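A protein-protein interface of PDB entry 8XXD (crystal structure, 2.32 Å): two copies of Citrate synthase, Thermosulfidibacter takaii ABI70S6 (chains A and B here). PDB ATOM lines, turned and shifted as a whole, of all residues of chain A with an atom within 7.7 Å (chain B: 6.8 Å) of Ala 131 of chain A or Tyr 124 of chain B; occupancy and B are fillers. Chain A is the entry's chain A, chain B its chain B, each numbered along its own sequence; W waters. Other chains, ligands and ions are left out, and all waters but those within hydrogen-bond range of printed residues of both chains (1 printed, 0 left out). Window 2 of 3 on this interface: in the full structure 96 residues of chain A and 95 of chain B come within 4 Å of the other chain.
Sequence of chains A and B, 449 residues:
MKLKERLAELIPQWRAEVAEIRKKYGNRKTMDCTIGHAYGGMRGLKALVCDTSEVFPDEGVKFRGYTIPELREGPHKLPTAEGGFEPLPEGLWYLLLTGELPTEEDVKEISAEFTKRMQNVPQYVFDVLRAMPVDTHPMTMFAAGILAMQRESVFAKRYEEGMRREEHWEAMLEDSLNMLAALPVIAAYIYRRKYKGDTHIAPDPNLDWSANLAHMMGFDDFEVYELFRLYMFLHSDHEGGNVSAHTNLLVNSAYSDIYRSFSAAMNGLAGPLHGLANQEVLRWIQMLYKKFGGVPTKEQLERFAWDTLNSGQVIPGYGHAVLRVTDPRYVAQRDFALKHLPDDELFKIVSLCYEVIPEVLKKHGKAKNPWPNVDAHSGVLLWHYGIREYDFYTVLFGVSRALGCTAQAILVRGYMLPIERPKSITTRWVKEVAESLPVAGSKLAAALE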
ATOM      1  N   VAL A 125      13.089   6.483 -15.290  1.00  0.00           N
ATOM      2  CA  VAL A 125      13.334   5.462 -14.254  1.00  0.00           C
ATOM      3  C   VAL A 125      13.448   6.121 -12.880  1.00  0.00           C
ATOM      4  O   VAL A 125      12.851   5.653 -11.931  1.00  0.00           O
ATOM      5  CB  VAL A 125      14.589   4.605 -14.528  1.00  0.00           C
ATOM      6  CG1 VAL A 125      14.987   3.794 -13.317  1.00  0.00           C
ATOM      7  CG2 VAL A 125      14.423   3.716 -15.738  1.00  0.00           C
ATOM      8  N   PHE A 126      14.189   7.234 -12.783  1.00  0.00           N
ATOM      9  CA  PHE A 126      14.261   8.056 -11.571  1.00  0.00           C
ATOM     10  C   PHE A 126      12.899   8.654 -11.183  1.00  0.00           C
ATOM     11  O   PHE A 126      12.565   8.673  -9.994  1.00  0.00           O
ATOM     12  CB  PHE A 126      15.336   9.146 -11.728  1.00  0.00           C
ATOM     13  CG  PHE A 126      16.682   8.587 -12.116  1.00  0.00           C
ATOM     14  CD1 PHE A 126      17.442   7.871 -11.206  1.00  0.00           C
ATOM     15  CD2 PHE A 126      17.164   8.706 -13.416  1.00  0.00           C
ATOM     16  CE1 PHE A 126      18.674   7.348 -11.567  1.00  0.00           C
ATOM     17  CE2 PHE A 126      18.398   8.184 -13.779  1.00  0.00           C
ATOM     18  CZ  PHE A 126      19.133   7.479 -12.864  1.00  0.00           C
ATOM     19  N   ASP A 127      12.090   9.131 -12.147  1.00  0.00           N
ATOM     20  CA  ASP A 127      10.726   9.561 -11.825  1.00  0.00           C
ATOM     21  C   ASP A 127       9.976   8.423 -11.131  1.00  0.00           C
ATOM     22  O   ASP A 127       9.316   8.635 -10.118  1.00  0.00           O
ATOM     23  CB  ASP A 127       9.933  10.020 -13.063  1.00  0.00           C
ATOM     24  CG  ASP A 127      10.593  11.176 -13.816  1.00  0.00           C
ATOM     25  OD1 ASP A 127      11.579  11.728 -13.268  1.00  0.00           O
ATOM     26  OD2 ASP A 127      10.141  11.527 -14.952  1.00  0.00           O
ATOM     27  N   VAL A 128      10.048   7.202 -11.681  1.00  0.00           N
ATOM     28  CA  VAL A 128       9.377   6.081 -11.047  1.00  0.00           C
ATOM     29  C   VAL A 128       9.932   5.851  -9.632  1.00  0.00           C
ATOM     30  O   VAL A 128       9.170   5.756  -8.663  1.00  0.00           O
ATOM     31  CB  VAL A 128       9.458   4.818 -11.920  1.00  0.00           C
ATOM     32  CG1 VAL A 128       9.143   3.573 -11.122  1.00  0.00           C
ATOM     33  CG2 VAL A 128       8.535   4.903 -13.128  1.00  0.00           C
ATOM     34  N   LEU A 129      11.263   5.823  -9.468  1.00  0.00           N
ATOM     35  CA  LEU A 129      11.825   5.608  -8.141  1.00  0.00           C
ATOM     36  C   LEU A 129      11.303   6.663  -7.163  1.00  0.00           C
ATOM     37  O   LEU A 129      10.970   6.324  -6.045  1.00  0.00           O
ATOM     38  CB  LEU A 129      13.353   5.600  -8.211  1.00  0.00           C
ATOM     39  CG  LEU A 129      13.935   4.390  -8.941  1.00  0.00           C
ATOM     40  CD1 LEU A 129      15.412   4.535  -9.139  1.00  0.00           C
ATOM     41  CD2 LEU A 129      13.664   3.112  -8.162  1.00  0.00           C
ATOM     42  N   ARG A 130      11.207   7.929  -7.576  1.00  0.00           N
ATOM     43  CA  ARG A 130      10.866   9.000  -6.665  1.00  0.00           C
ATOM     44  C   ARG A 130       9.374   8.996  -6.385  1.00  0.00           C
ATOM     45  O   ARG A 130       8.948   9.484  -5.348  1.00  0.00           O
ATOM     46  CB  ARG A 130      11.237  10.404  -7.176  1.00  0.00           C
ATOM     47  CG  ARG A 130      12.722  10.744  -7.119  1.00  0.00           C
ATOM     48  CD  ARG A 130      12.971  12.232  -7.360  1.00  0.00           C
ATOM     49  NE  ARG A 130      12.778  12.987  -6.147  1.00  0.00           N
ATOM     50  CZ  ARG A 130      13.630  12.983  -5.122  1.00  0.00           C
ATOM     51  NH1 ARG A 130      13.444  13.825  -4.117  1.00  0.00           N
ATOM     52  NH2 ARG A 130      14.708  12.202  -5.143  1.00  0.00           N
ATOM     53  N   ALA A 131       8.567   8.442  -7.271  1.00  0.00           N
ATOM     54  CA  ALA A 131       7.130   8.351  -6.972  1.00  0.00           C
ATOM     55  C   ALA A 131       6.782   7.279  -5.933  1.00  0.00           C
ATOM     56  O   ALA A 131       5.728   7.334  -5.301  1.00  0.00           O
ATOM     57  CB  ALA A 131       6.361   8.143  -8.229  1.00  0.00           C
ATOM     58  N   MET A 132       7.671   6.326  -5.699  1.00  0.00           N
ATOM     59  CA  MET A 132       7.474   5.402  -4.594  1.00  0.00           C
ATOM     60  C   MET A 132       7.775   6.095  -3.268  1.00  0.00           C
ATOM     61  O   MET A 132       8.765   6.819  -3.140  1.00  0.00           O
ATOM     62  CB  MET A 132       8.380   4.191  -4.776  1.00  0.00           C
ATOM     63  CG  MET A 132       8.106   3.503  -6.093  1.00  0.00           C
ATOM     64  SD  MET A 132       9.199   2.090  -6.415  1.00  0.00           S
ATOM     65  CE  MET A 132       8.083   0.877  -5.742  1.00  0.00           C
ATOM     66  N   PRO A 133       6.939   5.912  -2.219  1.00  0.00           N
ATOM     67  CA  PRO A 133       7.240   6.467  -0.913  1.00  0.00           C
ATOM     68  C   PRO A 133       8.588   5.963  -0.427  1.00  0.00           C
ATOM     69  O   PRO A 133       8.895   4.785  -0.579  1.00  0.00           O
ATOM     70  CB  PRO A 133       6.135   5.935  -0.015  1.00  0.00           C
ATOM     71  CG  PRO A 133       5.041   5.551  -0.953  1.00  0.00           C
ATOM     72  CD  PRO A 133       5.748   5.071  -2.196  1.00  0.00           C
ATOM     73  N   VAL A 134       9.391   6.879   0.123  1.00  0.00           N
ATOM     74  CA  VAL A 134      10.755   6.614   0.494  1.00  0.00           C
ATOM     75  C   VAL A 134      10.869   5.468   1.538  1.00  0.00           C
ATOM     76  O   VAL A 134      11.952   4.930   1.731  1.00  0.00           O
ATOM     77  CB  VAL A 134      11.369   7.917   1.044  1.00  0.00           C
ATOM     78  CG1 VAL A 134      10.798   8.273   2.418  1.00  0.00           C
ATOM     79  CG2 VAL A 134      12.897   7.833   1.142  1.00  0.00           C
ATOM     80  N   ASP A 135       9.795   5.118   2.256  1.00  0.00           N
ATOM     81  CA  ASP A 135       9.821   4.055   3.258  1.00  0.00           C
ATOM     82  C   ASP A 135       9.479   2.707   2.616  1.00  0.00           C
ATOM     83  O   ASP A 135       9.363   1.731   3.307  1.00  0.00           O
ATOM     84  CB  ASP A 135       8.864   4.307   4.448  1.00  0.00           C
ATOM     85  CG  ASP A 135       7.408   4.424   4.037  1.00  0.00           C
ATOM     86  OD1 ASP A 135       7.189   4.448   2.795  1.00  0.00           O
ATOM     87  OD2 ASP A 135       6.488   4.483   4.944  1.00  0.00           O
ATOM     88  N   THR A 136       9.302   2.648   1.295  1.00  0.00           N
ATOM     89  CA  THR A 136       9.118   1.395   0.600  1.00  0.00           C
ATOM     90  C   THR A 136      10.373   0.535   0.767  1.00  0.00           C
ATOM     91  O   THR A 136      11.486   1.049   0.829  1.00  0.00           O
ATOM     92  CB  THR A 136       8.814   1.664  -0.880  1.00  0.00           C
ATOM     93  OG1 THR A 136       7.608   2.425  -1.017  1.00  0.00           O
ATOM     94  CG2 THR A 136       8.723   0.376  -1.675  1.00  0.00           C
ATOM     95  N   MET A 141      11.634  -1.236  -4.505  1.00  0.00           N
ATOM     96  CA  MET A 141      12.101  -0.123  -5.308  1.00  0.00           C
ATOM     97  C   MET A 141      13.025  -0.636  -6.424  1.00  0.00           C
ATOM     98  O   MET A 141      12.930  -0.189  -7.566  1.00  0.00           O
ATOM     99  CB  MET A 141      12.898   0.854  -4.427  1.00  0.00           C
ATOM    100  CG  MET A 141      12.070   1.770  -3.556  1.00  0.00           C
ATOM    101  SD  MET A 141      13.160   2.897  -2.652  1.00  0.00           S
ATOM    102  CE  MET A 141      12.000   3.765  -1.605  1.00  0.00           C
ATOM    103  N   TYR A 189      20.879   4.968  -6.254  1.00  0.00           N
ATOM    104  CA  TYR A 189      19.840   5.981  -6.110  1.00  0.00           C
ATOM    105  C   TYR A 189      18.967   5.672  -4.884  1.00  0.00           C
ATOM    106  O   TYR A 189      18.746   6.531  -4.043  1.00  0.00           O
ATOM    107  CB  TYR A 189      19.025   6.108  -7.391  1.00  0.00           C
ATOM    108  CG  TYR A 189      18.142   7.327  -7.423  1.00  0.00           C
ATOM    109  CD1 TYR A 189      16.873   7.329  -6.858  1.00  0.00           C
ATOM    110  CD2 TYR A 189      18.609   8.500  -7.996  1.00  0.00           C
ATOM    111  CE1 TYR A 189      16.086   8.471  -6.876  1.00  0.00           C
ATOM    112  CE2 TYR A 189      17.841   9.645  -8.019  1.00  0.00           C
ATOM    113  CZ  TYR A 189      16.583   9.635  -7.452  1.00  0.00           C
ATOM    114  OH  TYR A 189      15.866  10.811  -7.558  1.00  0.00           O
ATOM    115  N   ARG A 193      18.817   7.945  -1.493  1.00  0.00           N
ATOM    116  CA  ARG A 193      17.525   8.558  -1.232  1.00  0.00           C
ATOM    117  C   ARG A 193      16.980   8.091   0.109  1.00  0.00           C
ATOM    118  O   ARG A 193      16.506   8.898   0.901  1.00  0.00           O
ATOM    119  CB  ARG A 193      16.524   8.240  -2.337  1.00  0.00           C
ATOM    120  CG  ARG A 193      15.159   8.812  -2.032  1.00  0.00           C
ATOM    121  CD  ARG A 193      14.171   8.687  -3.153  1.00  0.00           C
ATOM    122  NE  ARG A 193      12.913   9.313  -2.756  1.00  0.00           N
ATOM    123  CZ  ARG A 193      11.715   8.731  -2.802  1.00  0.00           C
ATOM    124  NH1 ARG A 193      11.593   7.481  -3.212  1.00  0.00           N
ATOM    125  NH2 ARG A 193      10.640   9.414  -2.458  1.00  0.00           N
ATOM    126  N   VAL B 121      -6.963   2.067  -3.096  1.00  0.00           N
ATOM    127  CA  VAL B 121      -5.705   2.030  -3.833  1.00  0.00           C
ATOM    128  C   VAL B 121      -4.900   3.265  -3.455  1.00  0.00           C
ATOM    129  O   VAL B 121      -5.390   4.384  -3.495  1.00  0.00           O
ATOM    130  CB  VAL B 121      -5.949   1.931  -5.336  1.00  0.00           C
ATOM    131  CG1 VAL B 121      -4.659   1.844  -6.139  1.00  0.00           C
ATOM    132  CG2 VAL B 121      -6.829   0.725  -5.630  1.00  0.00           C
ATOM    133  N   PRO B 122      -3.662   3.121  -2.959  1.00  0.00           N
ATOM    134  CA  PRO B 122      -2.874   4.295  -2.614  1.00  0.00           C
ATOM    135  C   PRO B 122      -2.726   5.279  -3.764  1.00  0.00           C
ATOM    136  O   PRO B 122      -2.452   4.867  -4.902  1.00  0.00           O
ATOM    137  CB  PRO B 122      -1.490   3.728  -2.269  1.00  0.00           C
ATOM    138  CG  PRO B 122      -1.794   2.304  -1.796  1.00  0.00           C
ATOM    139  CD  PRO B 122      -3.033   1.862  -2.545  1.00  0.00           C
ATOM    140  N   GLN B 123      -2.772   6.582  -3.424  1.00  0.00           N
ATOM    141  CA  GLN B 123      -2.484   7.631  -4.398  1.00  0.00           C
ATOM    142  C   GLN B 123      -1.127   7.400  -5.054  1.00  0.00           C
ATOM    143  O   GLN B 123      -0.988   7.618  -6.244  1.00  0.00           O
ATOM    144  CB  GLN B 123      -2.558   8.990  -3.712  1.00  0.00           C
ATOM    145  CG  GLN B 123      -2.314  10.160  -4.637  1.00  0.00           C
ATOM    146  CD  GLN B 123      -3.418  10.295  -5.652  1.00  0.00           C
ATOM    147  OE1 GLN B 123      -4.580  10.420  -5.281  1.00  0.00           O
ATOM    148  NE2 GLN B 123      -3.075  10.278  -6.939  1.00  0.00           N
ATOM    149  N   TYR B 124      -0.118   6.940  -4.297  1.00  0.00           N
ATOM    150  CA  TYR B 124       1.228   6.781  -4.828  1.00  0.00           C
ATOM    151  C   TYR B 124       1.286   5.725  -5.922  1.00  0.00           C
ATOM    152  O   TYR B 124       2.166   5.805  -6.785  1.00  0.00           O
ATOM    153  CB  TYR B 124       2.261   6.536  -3.717  1.00  0.00           C
ATOM    154  CG  TYR B 124       2.128   5.218  -3.012  1.00  0.00           C
ATOM    155  CD1 TYR B 124       2.551   4.050  -3.623  1.00  0.00           C
ATOM    156  CD2 TYR B 124       1.567   5.121  -1.740  1.00  0.00           C
ATOM    157  CE1 TYR B 124       2.435   2.817  -2.996  1.00  0.00           C
ATOM    158  CE2 TYR B 124       1.412   3.891  -1.113  1.00  0.00           C
ATOM    159  CZ  TYR B 124       1.838   2.730  -1.750  1.00  0.00           C
ATOM    160  OH  TYR B 124       1.657   1.462  -1.204  1.00  0.00           O
ATOM    161  N   VAL B 125       0.349   4.764  -5.944  1.00  0.00           N
ATOM    162  CA  VAL B 125       0.300   3.818  -7.043  1.00  0.00           C
ATOM    163  C   VAL B 125       0.036   4.576  -8.336  1.00  0.00           C
ATOM    164  O   VAL B 125       0.664   4.332  -9.365  1.00  0.00           O
ATOM    165  CB  VAL B 125      -0.729   2.694  -6.798  1.00  0.00           C
ATOM    166  CG1 VAL B 125      -0.964   1.813  -8.001  1.00  0.00           C
ATOM    167  CG2 VAL B 125      -0.333   1.837  -5.634  1.00  0.00           C
ATOM    168  N   PHE B 126      -0.906   5.508  -8.308  1.00  0.00           N
ATOM    169  CA  PHE B 126      -1.158   6.297  -9.505  1.00  0.00           C
ATOM    170  C   PHE B 126       0.055   7.138  -9.875  1.00  0.00           C
ATOM    171  O   PHE B 126       0.299   7.337 -11.047  1.00  0.00           O
ATOM    172  CB  PHE B 126      -2.406   7.159  -9.316  1.00  0.00           C
ATOM    173  CG  PHE B 126      -3.597   6.297  -9.004  1.00  0.00           C
ATOM    174  CD1 PHE B 126      -4.168   5.527  -9.990  1.00  0.00           C
ATOM    175  CD2 PHE B 126      -4.065   6.180  -7.707  1.00  0.00           C
ATOM    176  CE1 PHE B 126      -5.241   4.705  -9.708  1.00  0.00           C
ATOM    177  CE2 PHE B 126      -5.146   5.368  -7.420  1.00  0.00           C
ATOM    178  CZ  PHE B 126      -5.740   4.642  -8.424  1.00  0.00           C
ATOM    179  N   ASP B 127       0.754   7.705  -8.882  1.00  0.00           N
ATOM    180  CA  ASP B 127       1.937   8.489  -9.147  1.00  0.00           C
ATOM    181  C   ASP B 127       2.944   7.601  -9.870  1.00  0.00           C
ATOM    182  O   ASP B 127       3.545   8.025 -10.837  1.00  0.00           O
ATOM    183  CB  ASP B 127       2.545   9.057  -7.861  1.00  0.00           C
ATOM    184  CG  ASP B 127       1.654  10.002  -7.063  1.00  0.00           C
ATOM    185  OD1 ASP B 127       0.651  10.489  -7.613  1.00  0.00           O
ATOM    186  OD2 ASP B 127       1.988  10.268  -5.881  1.00  0.00           O
ATOM    187  N   VAL B 128       3.098   6.359  -9.427  1.00  0.00           N
ATOM    188  CA  VAL B 128       4.031   5.451 -10.073  1.00  0.00           C
ATOM    189  C   VAL B 128       3.623   5.230 -11.527  1.00  0.00           C
ATOM    190  O   VAL B 128       4.465   5.331 -12.427  1.00  0.00           O
ATOM    191  CB  VAL B 128       4.135   4.113  -9.324  1.00  0.00           C
ATOM    192  CG1 VAL B 128       4.673   3.005 -10.205  1.00  0.00           C
ATOM    193  CG2 VAL B 128       4.977   4.245  -8.070  1.00  0.00           C
ATOM    194  N   LEU B 129       2.331   4.945 -11.746  1.00  0.00           N
ATOM    195  CA  LEU B 129       1.788   4.725 -13.080  1.00  0.00           C
ATOM    196  C   LEU B 129       1.978   5.922 -14.005  1.00  0.00           C
ATOM    197  O   LEU B 129       2.365   5.726 -15.146  1.00  0.00           O
ATOM    198  CB  LEU B 129       0.295   4.382 -12.964  1.00  0.00           C
ATOM    199  CG  LEU B 129       0.007   2.988 -12.416  1.00  0.00           C
ATOM    200  CD1 LEU B 129      -1.454   2.834 -12.069  1.00  0.00           C
ATOM    201  CD2 LEU B 129       0.432   1.931 -13.416  1.00  0.00           C
ATOM    202  N   ALA B 131       4.261   8.213 -13.776  1.00  0.00           N
ATOM    203  CA  ALA B 131       5.675   8.459 -14.008  1.00  0.00           C
ATOM    204  C   ALA B 131       6.225   7.604 -15.164  1.00  0.00           C
ATOM    205  O   ALA B 131       7.295   7.880 -15.692  1.00  0.00           O
ATOM    206  CB  ALA B 131       6.391   8.158 -12.719  1.00  0.00           C
ATOM    207  N   GLY B 145       2.459  -1.355 -11.196  1.00  0.00           N
ATOM    208  CA  GLY B 145       1.513  -0.790 -10.238  1.00  0.00           C
ATOM    209  C   GLY B 145       1.302  -1.726  -9.052  1.00  0.00           C
ATOM    210  O   GLY B 145       1.342  -1.314  -7.881  1.00  0.00           O
ATOM    211  N   ALA B 148       4.293  -1.821  -6.757  1.00  0.00           N
ATOM    212  CA  ALA B 148       4.437  -0.614  -5.948  1.00  0.00           C
ATOM    213  C   ALA B 148       3.525  -0.714  -4.724  1.00  0.00           C
ATOM    214  O   ALA B 148       3.780  -0.120  -3.680  1.00  0.00           O
ATOM    215  CB  ALA B 148       4.119   0.624  -6.727  1.00  0.00           C
ATOM    216  N   MET B 149       2.484  -1.535  -4.840  1.00  0.00           N
ATOM    217  CA  MET B 149       1.531  -1.620  -3.768  1.00  0.00           C
ATOM    218  C   MET B 149       2.064  -2.580  -2.703  1.00  0.00           C
ATOM    219  O   MET B 149       1.515  -2.666  -1.623  1.00  0.00           O
ATOM    220  CB  MET B 149       0.188  -2.022  -4.339  1.00  0.00           C
ATOM    221  CG  MET B 149      -0.927  -1.832  -3.401  1.00  0.00           C
ATOM    222  SD  MET B 149      -2.500  -1.914  -4.296  1.00  0.00           S
ATOM    223  CE  MET B 149      -3.529  -1.978  -2.825  1.00  0.00           C
ATOM    224  N   GLN B 150       3.242  -3.169  -2.930  1.00  0.00           N
ATOM    225  CA  GLN B 150       3.823  -4.052  -1.949  1.00  0.00           C
ATOM    226  C   GLN B 150       4.002  -3.365  -0.597  1.00  0.00           C
ATOM    227  O   GLN B 150       4.034  -4.044   0.418  1.00  0.00           O
ATOM    228  CB  GLN B 150       5.141  -4.615  -2.467  1.00  0.00           C
ATOM    229  CG  GLN B 150       5.726  -5.699  -1.562  1.00  0.00           C
ATOM    230  CD  GLN B 150       6.553  -5.124  -0.440  1.00  0.00           C
ATOM    231  OE1 GLN B 150       7.111  -4.024  -0.550  1.00  0.00           O
ATOM    232  NE2 GLN B 150       6.662  -5.871   0.652  1.00  0.00           N
ATOM    233  N   ARG B 151       4.106  -2.025  -0.588  1.00  0.00           N
ATOM    234  CA  ARG B 151       4.293  -1.243   0.626  1.00  0.00           C
ATOM    235  C   ARG B 151       3.166  -1.509   1.628  1.00  0.00           C
ATOM    236  O   ARG B 151       3.392  -1.441   2.824  1.00  0.00           O
ATOM    237  CB  ARG B 151       4.380   0.264   0.329  1.00  0.00           C
ATOM    238  CG  ARG B 151       4.419   1.142   1.588  1.00  0.00           C
ATOM    239  CD  ARG B 151       4.447   2.610   1.195  1.00  0.00           C
ATOM    240  NE  ARG B 151       4.565   3.585   2.283  1.00  0.00           N
ATOM    241  CZ  ARG B 151       3.557   4.034   3.024  1.00  0.00           C
ATOM    242  NH1 ARG B 151       2.322   3.678   2.726  1.00  0.00           N
ATOM    243  NH2 ARG B 151       3.793   4.833   4.059  1.00  0.00           N
ATOM    244  N   GLU B 152       1.981  -1.847   1.136  1.00  0.00           N
ATOM    245  CA  GLU B 152       0.835  -2.170   1.974  1.00  0.00           C
ATOM    246  C   GLU B 152       0.772  -3.641   2.413  1.00  0.00           C
ATOM    247  O   GLU B 152      -0.240  -4.054   2.960  1.00  0.00           O
ATOM    248  CB  GLU B 152      -0.437  -1.838   1.179  1.00  0.00           C
ATOM    249  CG  GLU B 152      -0.496  -0.385   0.712  1.00  0.00           C
ATOM    250  CD  GLU B 152       0.043   0.682   1.670  1.00  0.00           C
ATOM    251  OE1 GLU B 152       0.878   1.500   1.247  1.00  0.00           O
ATOM    252  OE2 GLU B 152      -0.330   0.674   2.857  1.00  0.00           O
HETATM  253  O   HOH W   1       4.411   9.596  -4.718  1.00  0.00           O
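OD1 of Asp 135 of chain A is in salt-bridge range of NE of Arg 151 of chain B (2.8 Å).
The backbone carbonyl oxygen of Pro 133 of chain A lies within hydrogen-bond range of the side-chain hydroxyl of Thr 136 of chain A (2.7 Å). The side-chain hydroxyl (OH) of Tyr 124 of chain B lies within hydrogen-bond range of the side-chain carboxylate (OE1) of Glu 152 of chain B, 2.6 Å away. OE1 of Glu 152 of chain B lies within salt-bridge range of NH1 of Arg 151 of chain B. O of Met 132 of chain A sits at hydrogen-bond distance from NH1 of Arg 193 of chain A (2.9 Å).
C of Asp 127 of chain A touches CB of Ala 131 of chain B, at 3.9 Å. CG2 of Val 128 of chain A touches CB of Ala 131 of chain B (3.9 Å). O of Ala 131 of chain A touches CB of Tyr 124 of chain B, 3.9 Å away. C of Asp 127 of chain B touches CB of Ala 131 of chain A (3.8 Å). Ala 131 of chain A touches Val 128 of chain B (CB to N, 3.9 Å). Met 132 of chain A touches Val 128 of chain B. Met 132 of chain A touches Ala 148 of chain B (CE to CA, 3.9 Å). CG of Pro 133 of chain A touches CG of Tyr 124 of chain B (3.6 Å). Arg 151 of chain B touches Pro 133 of chain A. Thr 136 of chain A touches Arg 151 of chain B.
Ala 131 of chain A touches three residues of chain B. Tyr 124 of chain B touches just these residues of chain A: Ala 131 and Pro 133. Of the printed residues of chain A, Arg 151 of chain B touches Pro 133 (3.6 Å), Asp 135 (2.8 Å) and Thr 136 (3.9 Å). Of the printed residues of chain A, Val 128 of chain B touches Ala 131 and Met 132. Of the printed residues of chain B, Asp 127 of chain A touches Ala 131. Of the printed residues of chain A, Ala 131 of chain B touches Asp 127 and Val 128. Arg 193 of chain A touches none of the printed residues of chain B. Val 134 of chain A touches none of the printed residues of chain B. The nearest residue of chain A that does not touch Tyr 124 of chain B is Met 132 of chain A (5.2 Å).
Of the 15 printed residues of chain A, 7 touch a printed residue of chain B. Hydrophobic or aromatic side chains of chain A within 4 Å of the printed part of chain B: Val 128, Ala 131, Met 132 and Pro 133. Of the 16 printed residues of chain B, 6 touch a printed residue of chain A. Hydrophobic or aromatic side chains of chain B within 4 Å of the printed part of chain A: Tyr 124, Val 128 and Ala 131. Along chain B the printed residues that touch a printed residue of chain A span positions 124 to 151. Among the printed residues, 11 pairs touch across the chains.
Asp 127 of chain A touches Ala 131 of chain B, and with the chains exchanged Ala 131 of chain A touches Asp 127 of chain B. Val 128 of chain A touches Ala 131 of chain B, and with the chains exchanged Ala 131 of chain A touches Val 128 of chain B. Positions printed for both chains: 125, 126, 127, 128, 129 and 131. Of the 11 pairs that touch across the chains among the printed residues, 4 have their exchanged pair printed and touching as well.
Water W1 lies within hydrogen-bond range of the backbone carbonyl oxygen (O) of Ala 131 of chain A (2.7 Å) and the side-chain carboxylate (OD2) of Asp 127 of chain B (2.8 Å).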
